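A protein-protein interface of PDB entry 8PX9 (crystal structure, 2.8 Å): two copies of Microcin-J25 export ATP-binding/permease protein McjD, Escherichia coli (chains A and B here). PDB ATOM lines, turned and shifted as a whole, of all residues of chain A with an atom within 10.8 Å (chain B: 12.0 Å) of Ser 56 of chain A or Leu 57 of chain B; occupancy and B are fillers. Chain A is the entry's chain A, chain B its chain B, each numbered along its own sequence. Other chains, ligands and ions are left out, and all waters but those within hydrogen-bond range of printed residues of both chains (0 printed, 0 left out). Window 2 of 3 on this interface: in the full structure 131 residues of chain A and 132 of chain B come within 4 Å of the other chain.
The backbone carbonyl oxygen (O) of Leu 53 of chain B lies close to the backbone carbonyl oxygen (O) of Leu 53 of chain A (3.1 Å).
The backbone carbonyl oxygen (O) of Ser 56 of chain B lies close to the backbone carbonyl oxygen (O) of Ser 54 of chain A (3.3 Å).
Among the printed residues, pairs that only touch across the chains: Ile 283 of chain A with Leu 65 of chain B (3.5 Å), Leu 65 of chain A with Ile 283 of chain B (3.5 Å), Gly 55 of chain A with Leu 57 of chain B (3.5 Å), Leu 57 of chain A with Gly 55 of chain B (3.6 Å), Ser 54 of chain A with Leu 57 of chain B (3.6 Å), Leu 53 of chain A with Ile 283 of chain B (3.7 Å), Tyr 62 of chain A with Ile 283 of chain B (3.7 Å), Ile 283 of chain A with Tyr 62 of chain B (3.8 Å), Leu 53 of chain A with Ser 54 of chain B (3.8 Å), Leu 53 of chain A with Gly 55 of chain B (3.9 Å), Ser 54 of chain A with Leu 53 of chain B (3.9 Å), Ser 56 of chain A with Leu 57 of chain B (3.9 Å) and Ser 54 of chain A with Phe 60 of chain B (3.95 Å).
Of the 17 printed residues of chain B, 9 touch a printed residue of chain A.
Hydrophobic or aromatic side chains of chain B within 4 Å of the printed part of chain A: Leu 53, Leu 57, Phe 60, Tyr 62, Leu 65 and Ile 283.
Of the 19 printed residues of chain A, 8 touch a printed residue of chain B.
Hydrophobic or aromatic side chains of chain A that line the printed part of chain B: Leu 53, Leu 57, Tyr 62, Leu 65 and Ile 283.
Among the printed residues, 15 pairs touch across the chains.
The side-chain hydroxyl (OG) of Ser 54 of chain B sits close to the backbone carbonyl oxygen (O) of Thr 50 of chain B.
The backbone carbonyl oxygen (O) of Asp 51 of chain B sits at hydrogen-bond distance from the side-chain hydroxyl (OG) of Ser 54 of chain B (3.1 Å).
The backbone NH (N) of Asn 59 of chain B is in hydrogen-bond range of the side-chain hydroxyl (OG) of Ser 56 of chain B (3.0 Å).
The side-chain hydroxyl (OG) of Ser 56 of chain B lies within hydrogen-bond range of the backbone NH (N) of Phe 60 of chain B (3.1 Å).
Leu 53 of chain A touches its own counterpart, Leu 53 of chain B.
Leu 53 of chain A touches Gly 55 of chain B, but with the chains exchanged Gly 55 of chain A does not touch Leu 53 of chain B (5.8 Å).
Ser 56 of chain A touches Leu 57 of chain B, but with the chains exchanged Leu 57 of chain A does not touch Ser 56 of chain B (6.1 Å).
Tyr 62 of chain A touches Ile 283 of chain B, and with the chains exchanged Ile 283 of chain A touches Tyr 62 of chain B.
Of the 15 pairs that touch across the chains among the printed residues, 9 have their exchanged pair printed and touching as well.
Ser 56 of chain A touches one residue of chain B.
Leu 57 of chain B touches just these residues of chain A: Ser 54, Gly 55 and Ser 56.
No residue of chain B comes within 4 Å of Leu 52 of chain A.
Of chain B, only Leu 53 (3.9 Å), Ser 56 (3.3 Å), Leu 57 (3.6 Å) and Phe 60 (3.95 Å) come within 4 Å of Ser 54 of chain A.
Gly 55 of chain A touches just one residue of chain B: Leu 57.
Of chain B, only Gly 55 (3.6 Å) comes within 4 Å of Leu 57 of chain A.
No residue of chain B comes within 4 Å of Ser 58 of chain A.
Ser 56 of chain B touches just one residue of chain A: Ser 54.
No residue of chain A comes within 4 Å of Ser 58 of chain B.
Printed residues of chain A within 4 Å of Leu 53 of chain B: Leu 53 (3.1 Å) and Ser 54 (3.9 Å).
Of the printed residues of chain A, Tyr 62 of chain B touches Ile 283.
Of the printed residues of chain B, Tyr 62 of chain A touches Ile 283.
Of the printed residues of chain B, Leu 65 of chain A touches Ile 283 (3.5 Å).
Phe 60 of chain A touches none of the printed residues of chain B.
Asp 51 of chain B touches none of the printed residues of chain A.
The nearest printed residue of chain A that does not touch Leu 53 of chain B is Thr 50 of chain A (4.04 Å).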
ATOM      1  N   LYS A  48      11.130   6.200 -13.076  1.00  0.00           N
ATOM      2  CA  LYS A  48       9.693   6.012 -13.275  1.00  0.00           C
ATOM      3  C   LYS A  48       9.324   4.539 -13.418  1.00  0.00           C
ATOM      4  O   LYS A  48       8.259   4.142 -12.981  1.00  0.00           O
ATOM      5  CB  LYS A  48       9.201   6.874 -14.447  1.00  0.00           C
ATOM      6  CG  LYS A  48       9.203   8.354 -14.066  1.00  0.00           C
ATOM      7  CD  LYS A  48       8.769   9.367 -15.106  1.00  0.00           C
ATOM      8  CE  LYS A  48       8.791  10.768 -14.520  1.00  0.00           C
ATOM      9  NZ  LYS A  48       8.275  11.807 -15.447  1.00  0.00           N
ATOM     10  N   ILE A  49      10.206   3.728 -14.014  1.00  0.00           N
ATOM     11  CA  ILE A  49      10.025   2.277 -14.118  1.00  0.00           C
ATOM     12  C   ILE A  49      10.105   1.694 -12.697  1.00  0.00           C
ATOM     13  O   ILE A  49       9.240   0.924 -12.337  1.00  0.00           O
ATOM     14  CB  ILE A  49      11.053   1.642 -15.091  1.00  0.00           C
ATOM     15  CG1 ILE A  49      10.674   1.976 -16.544  1.00  0.00           C
ATOM     16  CG2 ILE A  49      11.207   0.137 -14.887  1.00  0.00           C
ATOM     17  CD1 ILE A  49      11.758   1.829 -17.564  1.00  0.00           C
ATOM     18  N   THR A  50      11.153   2.073 -11.952  1.00  0.00           N
ATOM     19  CA  THR A  50      11.449   1.493 -10.655  1.00  0.00           C
ATOM     20  C   THR A  50      10.315   1.696  -9.654  1.00  0.00           C
ATOM     21  O   THR A  50       9.925   0.735  -9.002  1.00  0.00           O
ATOM     22  CB  THR A  50      12.799   1.973 -10.117  1.00  0.00           C
ATOM     23  OG1 THR A  50      13.772   1.535 -11.068  1.00  0.00           O
ATOM     24  CG2 THR A  50      13.183   1.380  -8.774  1.00  0.00           C
ATOM     25  N   ASP A  51       9.810   2.928  -9.543  1.00  0.00           N
ATOM     26  CA  ASP A  51       8.752   3.256  -8.572  1.00  0.00           C
ATOM     27  C   ASP A  51       7.417   2.584  -8.950  1.00  0.00           C
ATOM     28  O   ASP A  51       6.685   2.140  -8.090  1.00  0.00           O
ATOM     29  CB  ASP A  51       8.619   4.766  -8.352  1.00  0.00           C
ATOM     30  CG  ASP A  51       8.300   5.612  -9.568  1.00  0.00           C
ATOM     31  OD1 ASP A  51       7.987   5.046 -10.625  1.00  0.00           O
ATOM     32  OD2 ASP A  51       8.556   6.804  -9.468  1.00  0.00           O
ATOM     33  N   LEU A  52       7.106   2.561 -10.257  1.00  0.00           N
ATOM     34  CA  LEU A  52       5.931   1.932 -10.817  1.00  0.00           C
ATOM     35  C   LEU A  52       5.832   0.453 -10.440  1.00  0.00           C
ATOM     36  O   LEU A  52       4.720  -0.016 -10.254  1.00  0.00           O
ATOM     37  CB  LEU A  52       5.972   2.163 -12.340  1.00  0.00           C
ATOM     38  CG  LEU A  52       4.797   1.723 -13.211  1.00  0.00           C
ATOM     39  CD1 LEU A  52       3.590   2.555 -12.939  1.00  0.00           C
ATOM     40  CD2 LEU A  52       5.176   1.785 -14.645  1.00  0.00           C
ATOM     41  N   LEU A  53       6.961  -0.291 -10.393  1.00  0.00           N
ATOM     42  CA  LEU A  53       7.047  -1.672  -9.971  1.00  0.00           C
ATOM     43  C   LEU A  53       6.673  -1.917  -8.497  1.00  0.00           C
ATOM     44  O   LEU A  53       6.005  -2.913  -8.210  1.00  0.00           O
ATOM     45  CB  LEU A  53       8.498  -2.150 -10.144  1.00  0.00           C
ATOM     46  CG  LEU A  53       9.126  -2.240 -11.524  1.00  0.00           C
ATOM     47  CD1 LEU A  53      10.606  -2.520 -11.366  1.00  0.00           C
ATOM     48  CD2 LEU A  53       8.475  -3.280 -12.405  1.00  0.00           C
ATOM     49  N   SER A  54       7.076  -0.989  -7.592  1.00  0.00           N
ATOM     50  CA  SER A  54       6.701  -1.049  -6.178  1.00  0.00           C
ATOM     51  C   SER A  54       5.207  -0.835  -5.993  1.00  0.00           C
ATOM     52  O   SER A  54       4.637  -1.436  -5.097  1.00  0.00           O
ATOM     53  CB  SER A  54       7.475  -0.115  -5.284  1.00  0.00           C
ATOM     54  OG  SER A  54       8.865  -0.379  -5.355  1.00  0.00           O
ATOM     55  N   GLY A  55       4.570  -0.001  -6.835  1.00  0.00           N
ATOM     56  CA  GLY A  55       3.167   0.313  -6.670  1.00  0.00           C
ATOM     57  C   GLY A  55       2.221  -0.789  -7.160  1.00  0.00           C
ATOM     58  O   GLY A  55       2.600  -1.954  -7.286  1.00  0.00           O
ATOM     59  N   SER A  56       0.970  -0.389  -7.419  1.00  0.00           N
ATOM     60  CA  SER A  56      -0.012  -1.252  -8.055  1.00  0.00           C
ATOM     61  C   SER A  56       0.373  -1.567  -9.493  1.00  0.00           C
ATOM     62  O   SER A  56       1.047  -0.791 -10.193  1.00  0.00           O
ATOM     63  CB  SER A  56      -1.383  -0.636  -8.057  1.00  0.00           C
ATOM     64  OG  SER A  56      -2.335  -1.611  -8.445  1.00  0.00           O
ATOM     65  N   LEU A  57      -0.134  -2.706 -10.002  1.00  0.00           N
ATOM     66  CA  LEU A  57       0.144  -3.148 -11.357  1.00  0.00           C
ATOM     67  C   LEU A  57      -1.170  -3.388 -12.100  1.00  0.00           C
ATOM     68  O   LEU A  57      -1.552  -4.517 -12.369  1.00  0.00           O
ATOM     69  CB  LEU A  57       1.034  -4.380 -11.268  1.00  0.00           C
ATOM     70  CG  LEU A  57       2.484  -4.007 -10.976  1.00  0.00           C
ATOM     71  CD1 LEU A  57       3.259  -5.196 -10.449  1.00  0.00           C
ATOM     72  CD2 LEU A  57       3.153  -3.397 -12.206  1.00  0.00           C
ATOM     73  N   SER A  58      -1.828  -2.268 -12.411  1.00  0.00           N
ATOM     74  CA  SER A  58      -3.053  -2.208 -13.197  1.00  0.00           C
ATOM     75  C   SER A  58      -2.738  -2.440 -14.675  1.00  0.00           C
ATOM     76  O   SER A  58      -1.580  -2.402 -15.072  1.00  0.00           O
ATOM     77  CB  SER A  58      -3.771  -0.891 -12.954  1.00  0.00           C
ATOM     78  OG  SER A  58      -2.862   0.181 -12.823  1.00  0.00           O
ATOM     79  N   ASN A  59      -3.783  -2.555 -15.512  1.00  0.00           N
ATOM     80  CA  ASN A  59      -3.659  -2.665 -16.977  1.00  0.00           C
ATOM     81  C   ASN A  59      -2.882  -1.450 -17.542  1.00  0.00           C
ATOM     82  O   ASN A  59      -1.948  -1.594 -18.350  1.00  0.00           O
ATOM     83  CB  ASN A  59      -5.056  -2.809 -17.564  1.00  0.00           C
ATOM     84  CG  ASN A  59      -5.077  -3.099 -19.049  1.00  0.00           C
ATOM     85  OD1 ASN A  59      -4.152  -3.687 -19.600  1.00  0.00           O
ATOM     86  ND2 ASN A  59      -6.149  -2.695 -19.698  1.00  0.00           N
ATOM     87  N   PHE A  60      -3.252  -0.247 -17.055  1.00  0.00           N
ATOM     88  CA  PHE A  60      -2.656   1.033 -17.470  1.00  0.00           C
ATOM     89  C   PHE A  60      -1.240   1.195 -16.884  1.00  0.00           C
ATOM     90  O   PHE A  60      -0.491   2.087 -17.311  1.00  0.00           O
ATOM     91  CB  PHE A  60      -3.671   2.180 -17.219  1.00  0.00           C
ATOM     92  CG  PHE A  60      -5.004   2.004 -17.911  1.00  0.00           C
ATOM     93  CD1 PHE A  60      -5.194   2.417 -19.226  1.00  0.00           C
ATOM     94  CD2 PHE A  60      -6.079   1.418 -17.245  1.00  0.00           C
ATOM     95  CE1 PHE A  60      -6.415   2.243 -19.854  1.00  0.00           C
ATOM     96  CE2 PHE A  60      -7.300   1.239 -17.880  1.00  0.00           C
ATOM     97  CZ  PHE A  60      -7.467   1.656 -19.182  1.00  0.00           C
ATOM     98  N   SER A  61      -0.893   0.468 -15.819  1.00  0.00           N
ATOM     99  CA  SER A  61       0.467   0.442 -15.298  1.00  0.00           C
ATOM    100  C   SER A  61       1.385  -0.410 -16.155  1.00  0.00           C
ATOM    101  O   SER A  61       2.551  -0.069 -16.207  1.00  0.00           O
ATOM    102  CB  SER A  61       0.541   0.012 -13.841  1.00  0.00           C
ATOM    103  OG  SER A  61      -0.234   0.881 -13.030  1.00  0.00           O
ATOM    104  N   TYR A  62       0.913  -1.502 -16.774  1.00  0.00           N
ATOM    105  CA  TYR A  62       1.739  -2.336 -17.643  1.00  0.00           C
ATOM    106  C   TYR A  62       1.972  -1.662 -18.984  1.00  0.00           C
ATOM    107  O   TYR A  62       3.095  -1.691 -19.514  1.00  0.00           O
ATOM    108  CB  TYR A  62       1.182  -3.757 -17.815  1.00  0.00           C
ATOM    109  CG  TYR A  62       1.424  -4.666 -16.620  1.00  0.00           C
ATOM    110  CD1 TYR A  62       2.702  -5.163 -16.346  1.00  0.00           C
ATOM    111  CD2 TYR A  62       0.398  -4.961 -15.709  1.00  0.00           C
ATOM    112  CE1 TYR A  62       2.948  -5.939 -15.224  1.00  0.00           C
ATOM    113  CE2 TYR A  62       0.643  -5.730 -14.583  1.00  0.00           C
ATOM    114  CZ  TYR A  62       1.916  -6.232 -14.346  1.00  0.00           C
ATOM    115  OH  TYR A  62       2.131  -7.008 -13.239  1.00  0.00           O
ATOM    116  N   GLU A  63       0.946  -1.017 -19.534  1.00  0.00           N
ATOM    117  CA  GLU A  63       1.036  -0.269 -20.790  1.00  0.00           C
ATOM    118  C   GLU A  63       2.017   0.913 -20.670  1.00  0.00           C
ATOM    119  O   GLU A  63       2.795   1.185 -21.580  1.00  0.00           O
ATOM    120  CB  GLU A  63      -0.354   0.201 -21.236  1.00  0.00           C
ATOM    121  CG  GLU A  63      -1.276  -0.914 -21.666  1.00  0.00           C
ATOM    122  CD  GLU A  63      -2.757  -0.586 -21.791  1.00  0.00           C
ATOM    123  OE1 GLU A  63      -3.173   0.577 -21.556  1.00  0.00           O
ATOM    124  OE2 GLU A  63      -3.523  -1.509 -22.145  1.00  0.00           O
ATOM    125  N   TYR A  64       2.003   1.607 -19.526  1.00  0.00           N
ATOM    126  CA  TYR A  64       2.903   2.705 -19.209  1.00  0.00           C
ATOM    127  C   TYR A  64       4.343   2.222 -19.007  1.00  0.00           C
ATOM    128  O   TYR A  64       5.276   2.923 -19.364  1.00  0.00           O
ATOM    129  CB  TYR A  64       2.404   3.466 -17.974  1.00  0.00           C
ATOM    130  CG  TYR A  64       3.142   4.760 -17.678  1.00  0.00           C
ATOM    131  CD1 TYR A  64       3.204   5.786 -18.618  1.00  0.00           C
ATOM    132  CD2 TYR A  64       3.715   4.988 -16.435  1.00  0.00           C
ATOM    133  CE1 TYR A  64       3.860   6.978 -18.344  1.00  0.00           C
ATOM    134  CE2 TYR A  64       4.378   6.171 -16.145  1.00  0.00           C
ATOM    135  CZ  TYR A  64       4.461   7.170 -17.106  1.00  0.00           C
ATOM    136  OH  TYR A  64       5.118   8.335 -16.813  1.00  0.00           O
ATOM    137  N   LEU A  65       4.517   1.023 -18.428  1.00  0.00           N
ATOM    138  CA  LEU A  65       5.817   0.391 -18.209  1.00  0.00           C
ATOM    139  C   LEU A  65       6.460   0.042 -19.545  1.00  0.00           C
ATOM    140  O   LEU A  65       7.645   0.260 -19.727  1.00  0.00           O
ATOM    141  CB  LEU A  65       5.645  -0.866 -17.347  1.00  0.00           C
ATOM    142  CG  LEU A  65       6.937  -1.576 -16.961  1.00  0.00           C
ATOM    143  CD1 LEU A  65       7.786  -0.710 -16.030  1.00  0.00           C
ATOM    144  CD2 LEU A  65       6.648  -2.915 -16.312  1.00  0.00           C
ATOM    145  N   ILE A 283      12.919   4.174  -3.474  1.00  0.00           N
ATOM    146  CA  ILE A 283      13.723   3.295  -4.337  1.00  0.00           C
ATOM    147  C   ILE A 283      13.897   3.929  -5.728  1.00  0.00           C
ATOM    148  O   ILE A 283      14.995   3.884  -6.285  1.00  0.00           O
ATOM    149  CB  ILE A 283      13.169   1.848  -4.409  1.00  0.00           C
ATOM    150  CG1 ILE A 283      12.984   1.237  -3.021  1.00  0.00           C
ATOM    151  CG2 ILE A 283      14.059   0.956  -5.287  1.00  0.00           C
ATOM    152  CD1 ILE A 283      14.244   1.192  -2.202  1.00  0.00           C
ATOM    153  N   ILE B  49      16.469  -7.753  -8.909  1.00  0.00           N
ATOM    154  CA  ILE B  49      16.023  -6.455  -8.398  1.00  0.00           C
ATOM    155  C   ILE B  49      14.586  -6.227  -8.861  1.00  0.00           C
ATOM    156  O   ILE B  49      13.743  -5.895  -8.037  1.00  0.00           O
ATOM    157  CB  ILE B  49      16.964  -5.297  -8.835  1.00  0.00           C
ATOM    158  CG1 ILE B  49      18.338  -5.378  -8.147  1.00  0.00           C
ATOM    159  CG2 ILE B  49      16.325  -3.900  -8.698  1.00  0.00           C
ATOM    160  CD1 ILE B  49      18.395  -4.944  -6.707  1.00  0.00           C
ATOM    161  N   THR B  50      14.340  -6.393 -10.168  1.00  0.00           N
ATOM    162  CA  THR B  50      13.031  -6.180 -10.768  1.00  0.00           C
ATOM    163  C   THR B  50      11.972  -7.097 -10.151  1.00  0.00           C
ATOM    164  O   THR B  50      10.908  -6.596  -9.822  1.00  0.00           O
ATOM    165  CB  THR B  50      13.098  -6.353 -12.288  1.00  0.00           C
ATOM    166  OG1 THR B  50      14.104  -5.471 -12.788  1.00  0.00           O
ATOM    167  CG2 THR B  50      11.792  -6.053 -12.983  1.00  0.00           C
ATOM    168  N   ASP B  51      12.282  -8.400  -9.980  1.00  0.00           N
ATOM    169  CA  ASP B  51      11.362  -9.372  -9.395  1.00  0.00           C
ATOM    170  C   ASP B  51      11.035  -9.087  -7.927  1.00  0.00           C
ATOM    171  O   ASP B  51       9.872  -9.194  -7.547  1.00  0.00           O
ATOM    172  CB  ASP B  51      11.850 -10.822  -9.561  1.00  0.00           C
ATOM    173  CG  ASP B  51      11.556 -11.420 -10.928  1.00  0.00           C
ATOM    174  OD1 ASP B  51      10.451 -11.140 -11.470  1.00  0.00           O
ATOM    175  OD2 ASP B  51      12.401 -12.208 -11.426  1.00  0.00           O
ATOM    176  N   LEU B  52      12.039  -8.707  -7.126  1.00  0.00           N
ATOM    177  CA  LEU B  52      11.863  -8.369  -5.715  1.00  0.00           C
ATOM    178  C   LEU B  52      10.882  -7.203  -5.529  1.00  0.00           C
ATOM    179  O   LEU B  52      10.035  -7.279  -4.636  1.00  0.00           O
ATOM    180  CB  LEU B  52      13.232  -8.036  -5.109  1.00  0.00           C
ATOM    181  CG  LEU B  52      13.302  -8.035  -3.590  1.00  0.00           C
ATOM    182  CD1 LEU B  52      13.307  -9.458  -3.054  1.00  0.00           C
ATOM    183  CD2 LEU B  52      14.480  -7.215  -3.065  1.00  0.00           C
ATOM    184  N   LEU B  53      10.971  -6.181  -6.396  1.00  0.00           N
ATOM    185  CA  LEU B  53      10.091  -5.016  -6.368  1.00  0.00           C
ATOM    186  C   LEU B  53       8.724  -5.334  -6.989  1.00  0.00           C
ATOM    187  O   LEU B  53       7.715  -4.857  -6.461  1.00  0.00           O
ATOM    188  CB  LEU B  53      10.734  -3.841  -7.114  1.00  0.00           C
ATOM    189  CG  LEU B  53      12.113  -3.373  -6.633  1.00  0.00           C
ATOM    190  CD1 LEU B  53      12.745  -2.482  -7.686  1.00  0.00           C
ATOM    191  CD2 LEU B  53      12.062  -2.635  -5.314  1.00  0.00           C
ATOM    192  N   SER B  54       8.707  -6.080  -8.119  1.00  0.00           N
ATOM    193  CA  SER B  54       7.506  -6.378  -8.895  1.00  0.00           C
ATOM    194  C   SER B  54       6.533  -7.226  -8.088  1.00  0.00           C
ATOM    195  O   SER B  54       6.910  -8.291  -7.591  1.00  0.00           O
ATOM    196  CB  SER B  54       7.776  -7.099 -10.200  1.00  0.00           C
ATOM    197  OG  SER B  54       8.108  -8.473 -10.002  1.00  0.00           O
ATOM    198  N   GLY B  55       5.294  -6.743  -7.971  1.00  0.00           N
ATOM    199  CA  GLY B  55       4.260  -7.481  -7.281  1.00  0.00           C
ATOM    200  C   GLY B  55       4.153  -7.041  -5.831  1.00  0.00           C
ATOM    201  O   GLY B  55       3.065  -6.634  -5.423  1.00  0.00           O
ATOM    202  N   SER B  56       5.264  -7.129  -5.073  1.00  0.00           N
ATOM    203  CA  SER B  56       5.268  -6.746  -3.667  1.00  0.00           C
ATOM    204  C   SER B  56       4.989  -5.247  -3.508  1.00  0.00           C
ATOM    205  O   SER B  56       5.557  -4.440  -4.232  1.00  0.00           O
ATOM    206  CB  SER B  56       6.559  -7.123  -2.981  1.00  0.00           C
ATOM    207  OG  SER B  56       6.470  -6.826  -1.583  1.00  0.00           O
ATOM    208  N   LEU B  57       4.108  -4.894  -2.567  1.00  0.00           N
ATOM    209  CA  LEU B  57       3.710  -3.517  -2.323  1.00  0.00           C
ATOM    210  C   LEU B  57       4.551  -2.990  -1.167  1.00  0.00           C
ATOM    211  O   LEU B  57       4.085  -2.825  -0.040  1.00  0.00           O
ATOM    212  CB  LEU B  57       2.204  -3.510  -2.065  1.00  0.00           C
ATOM    213  CG  LEU B  57       1.370  -3.735  -3.329  1.00  0.00           C
ATOM    214  CD1 LEU B  57       0.008  -4.340  -3.012  1.00  0.00           C
ATOM    215  CD2 LEU B  57       1.221  -2.425  -4.068  1.00  0.00           C
ATOM    216  N   SER B  58       5.837  -2.778  -1.469  1.00  0.00           N
ATOM    217  CA  SER B  58       6.875  -2.357  -0.531  1.00  0.00           C
ATOM    218  C   SER B  58       7.126  -3.330   0.638  1.00  0.00           C
ATOM    219  O   SER B  58       7.707  -2.916   1.641  1.00  0.00           O
ATOM    220  CB  SER B  58       6.649  -0.917  -0.093  1.00  0.00           C
ATOM    221  OG  SER B  58       6.751  -0.045  -1.206  1.00  0.00           O
ATOM    222  N   ASN B  59       6.752  -4.624   0.505  1.00  0.00           N
ATOM    223  CA  ASN B  59       6.960  -5.650   1.532  1.00  0.00           C
ATOM    224  C   ASN B  59       8.171  -6.557   1.253  1.00  0.00           C
ATOM    225  O   ASN B  59       8.423  -7.474   2.029  1.00  0.00           O
ATOM    226  CB  ASN B  59       5.669  -6.452   1.747  1.00  0.00           C
ATOM    227  CG  ASN B  59       4.537  -5.619   2.319  1.00  0.00           C
ATOM    228  OD1 ASN B  59       4.747  -4.693   3.104  1.00  0.00           O
ATOM    229  ND2 ASN B  59       3.314  -5.945   1.939  1.00  0.00           N
ATOM    230  N   PHE B  60       8.926  -6.311   0.168  1.00  0.00           N
ATOM    231  CA  PHE B  60      10.222  -6.923  -0.130  1.00  0.00           C
ATOM    232  C   PHE B  60      11.284  -6.604   0.932  1.00  0.00           C
ATOM    233  O   PHE B  60      11.207  -5.543   1.543  1.00  0.00           O
ATOM    234  CB  PHE B  60      10.694  -6.460  -1.511  1.00  0.00           C
ATOM    235  CG  PHE B  60      10.822  -4.967  -1.707  1.00  0.00           C
ATOM    236  CD1 PHE B  60      11.974  -4.291  -1.311  1.00  0.00           C
ATOM    237  CD2 PHE B  60       9.780  -4.226  -2.265  1.00  0.00           C
ATOM    238  CE1 PHE B  60      12.106  -2.924  -1.521  1.00  0.00           C
ATOM    239  CE2 PHE B  60       9.902  -2.854  -2.455  1.00  0.00           C
ATOM    240  CZ  PHE B  60      11.054  -2.200  -2.060  1.00  0.00           C
ATOM    241  N   SER B  61      12.277  -7.498   1.125  1.00  0.00           N
ATOM    242  CA  SER B  61      13.363  -7.253   2.075  1.00  0.00           C
ATOM    243  C   SER B  61      14.319  -6.188   1.519  1.00  0.00           C
ATOM    244  O   SER B  61      14.867  -6.349   0.426  1.00  0.00           O
ATOM    245  CB  SER B  61      14.096  -8.508   2.458  1.00  0.00           C
ATOM    246  OG  SER B  61      14.763  -9.065   1.349  1.00  0.00           O
ATOM    247  N   TYR B  62      14.444  -5.067   2.249  1.00  0.00           N
ATOM    248  CA  TYR B  62      15.308  -3.952   1.878  1.00  0.00           C
ATOM    249  C   TYR B  62      16.794  -4.334   1.941  1.00  0.00           C
ATOM    250  O   TYR B  62      17.569  -3.855   1.114  1.00  0.00           O
ATOM    251  CB  TYR B  62      15.021  -2.719   2.743  1.00  0.00           C
ATOM    252  CG  TYR B  62      13.829  -1.892   2.293  1.00  0.00           C
ATOM    253  CD1 TYR B  62      12.521  -2.314   2.498  1.00  0.00           C
ATOM    254  CD2 TYR B  62      14.016  -0.664   1.664  1.00  0.00           C
ATOM    255  CE1 TYR B  62      11.440  -1.527   2.108  1.00  0.00           C
ATOM    256  CE2 TYR B  62      12.945   0.122   1.246  1.00  0.00           C
ATOM    257  CZ  TYR B  62      11.647  -0.304   1.480  1.00  0.00           C
ATOM    258  OH  TYR B  62      10.590   0.452   1.061  1.00  0.00           O
ATOM    259  N   LEU B  65      17.732  -6.095  -1.240  1.00  0.00           N
ATOM    260  CA  LEU B  65      17.750  -5.108  -2.318  1.00  0.00           C
ATOM    261  C   LEU B  65      19.068  -4.333  -2.332  1.00  0.00           C
ATOM    262  O   LEU B  65      19.629  -4.123  -3.401  1.00  0.00           O
ATOM    263  CB  LEU B  65      16.557  -4.152  -2.165  1.00  0.00           C
ATOM    264  CG  LEU B  65      16.369  -3.085  -3.250  1.00  0.00           C
ATOM    265  CD1 LEU B  65      16.004  -3.712  -4.588  1.00  0.00           C
ATOM    266  CD2 LEU B  65      15.297  -2.073  -2.852  1.00  0.00           C
ATOM    267  N   VAL B 276       4.693  -9.521 -21.800  1.00  0.00           N
ATOM    268  CA  VAL B 276       4.416  -8.863 -20.523  1.00  0.00           C
ATOM    269  C   VAL B 276       3.007  -8.275 -20.492  1.00  0.00           C
ATOM    270  O   VAL B 276       2.388  -8.301 -19.422  1.00  0.00           O
ATOM    271  CB  VAL B 276       5.471  -7.829 -20.091  1.00  0.00           C
ATOM    272  CG1 VAL B 276       6.789  -8.515 -19.761  1.00  0.00           C
ATOM    273  CG2 VAL B 276       5.667  -6.660 -21.051  1.00  0.00           C
ATOM    274  N   ILE B 283       8.010  -9.343 -15.666  1.00  0.00           N
ATOM    275  CA  ILE B 283       8.756  -8.095 -15.850  1.00  0.00           C
ATOM    276  C   ILE B 283      10.249  -8.347 -15.593  1.00  0.00           C
ATOM    277  O   ILE B 283      11.077  -7.826 -16.342  1.00  0.00           O
ATOM    278  CB  ILE B 283       8.194  -6.931 -14.993  1.00  0.00           C
ATOM    279  CG1 ILE B 283       6.695  -6.698 -15.227  1.00  0.00           C
ATOM    280  CG2 ILE B 283       8.978  -5.635 -15.218  1.00  0.00           C
ATOM    281  CD1 ILE B 283       6.331  -6.386 -16.662  1.00  0.00           C
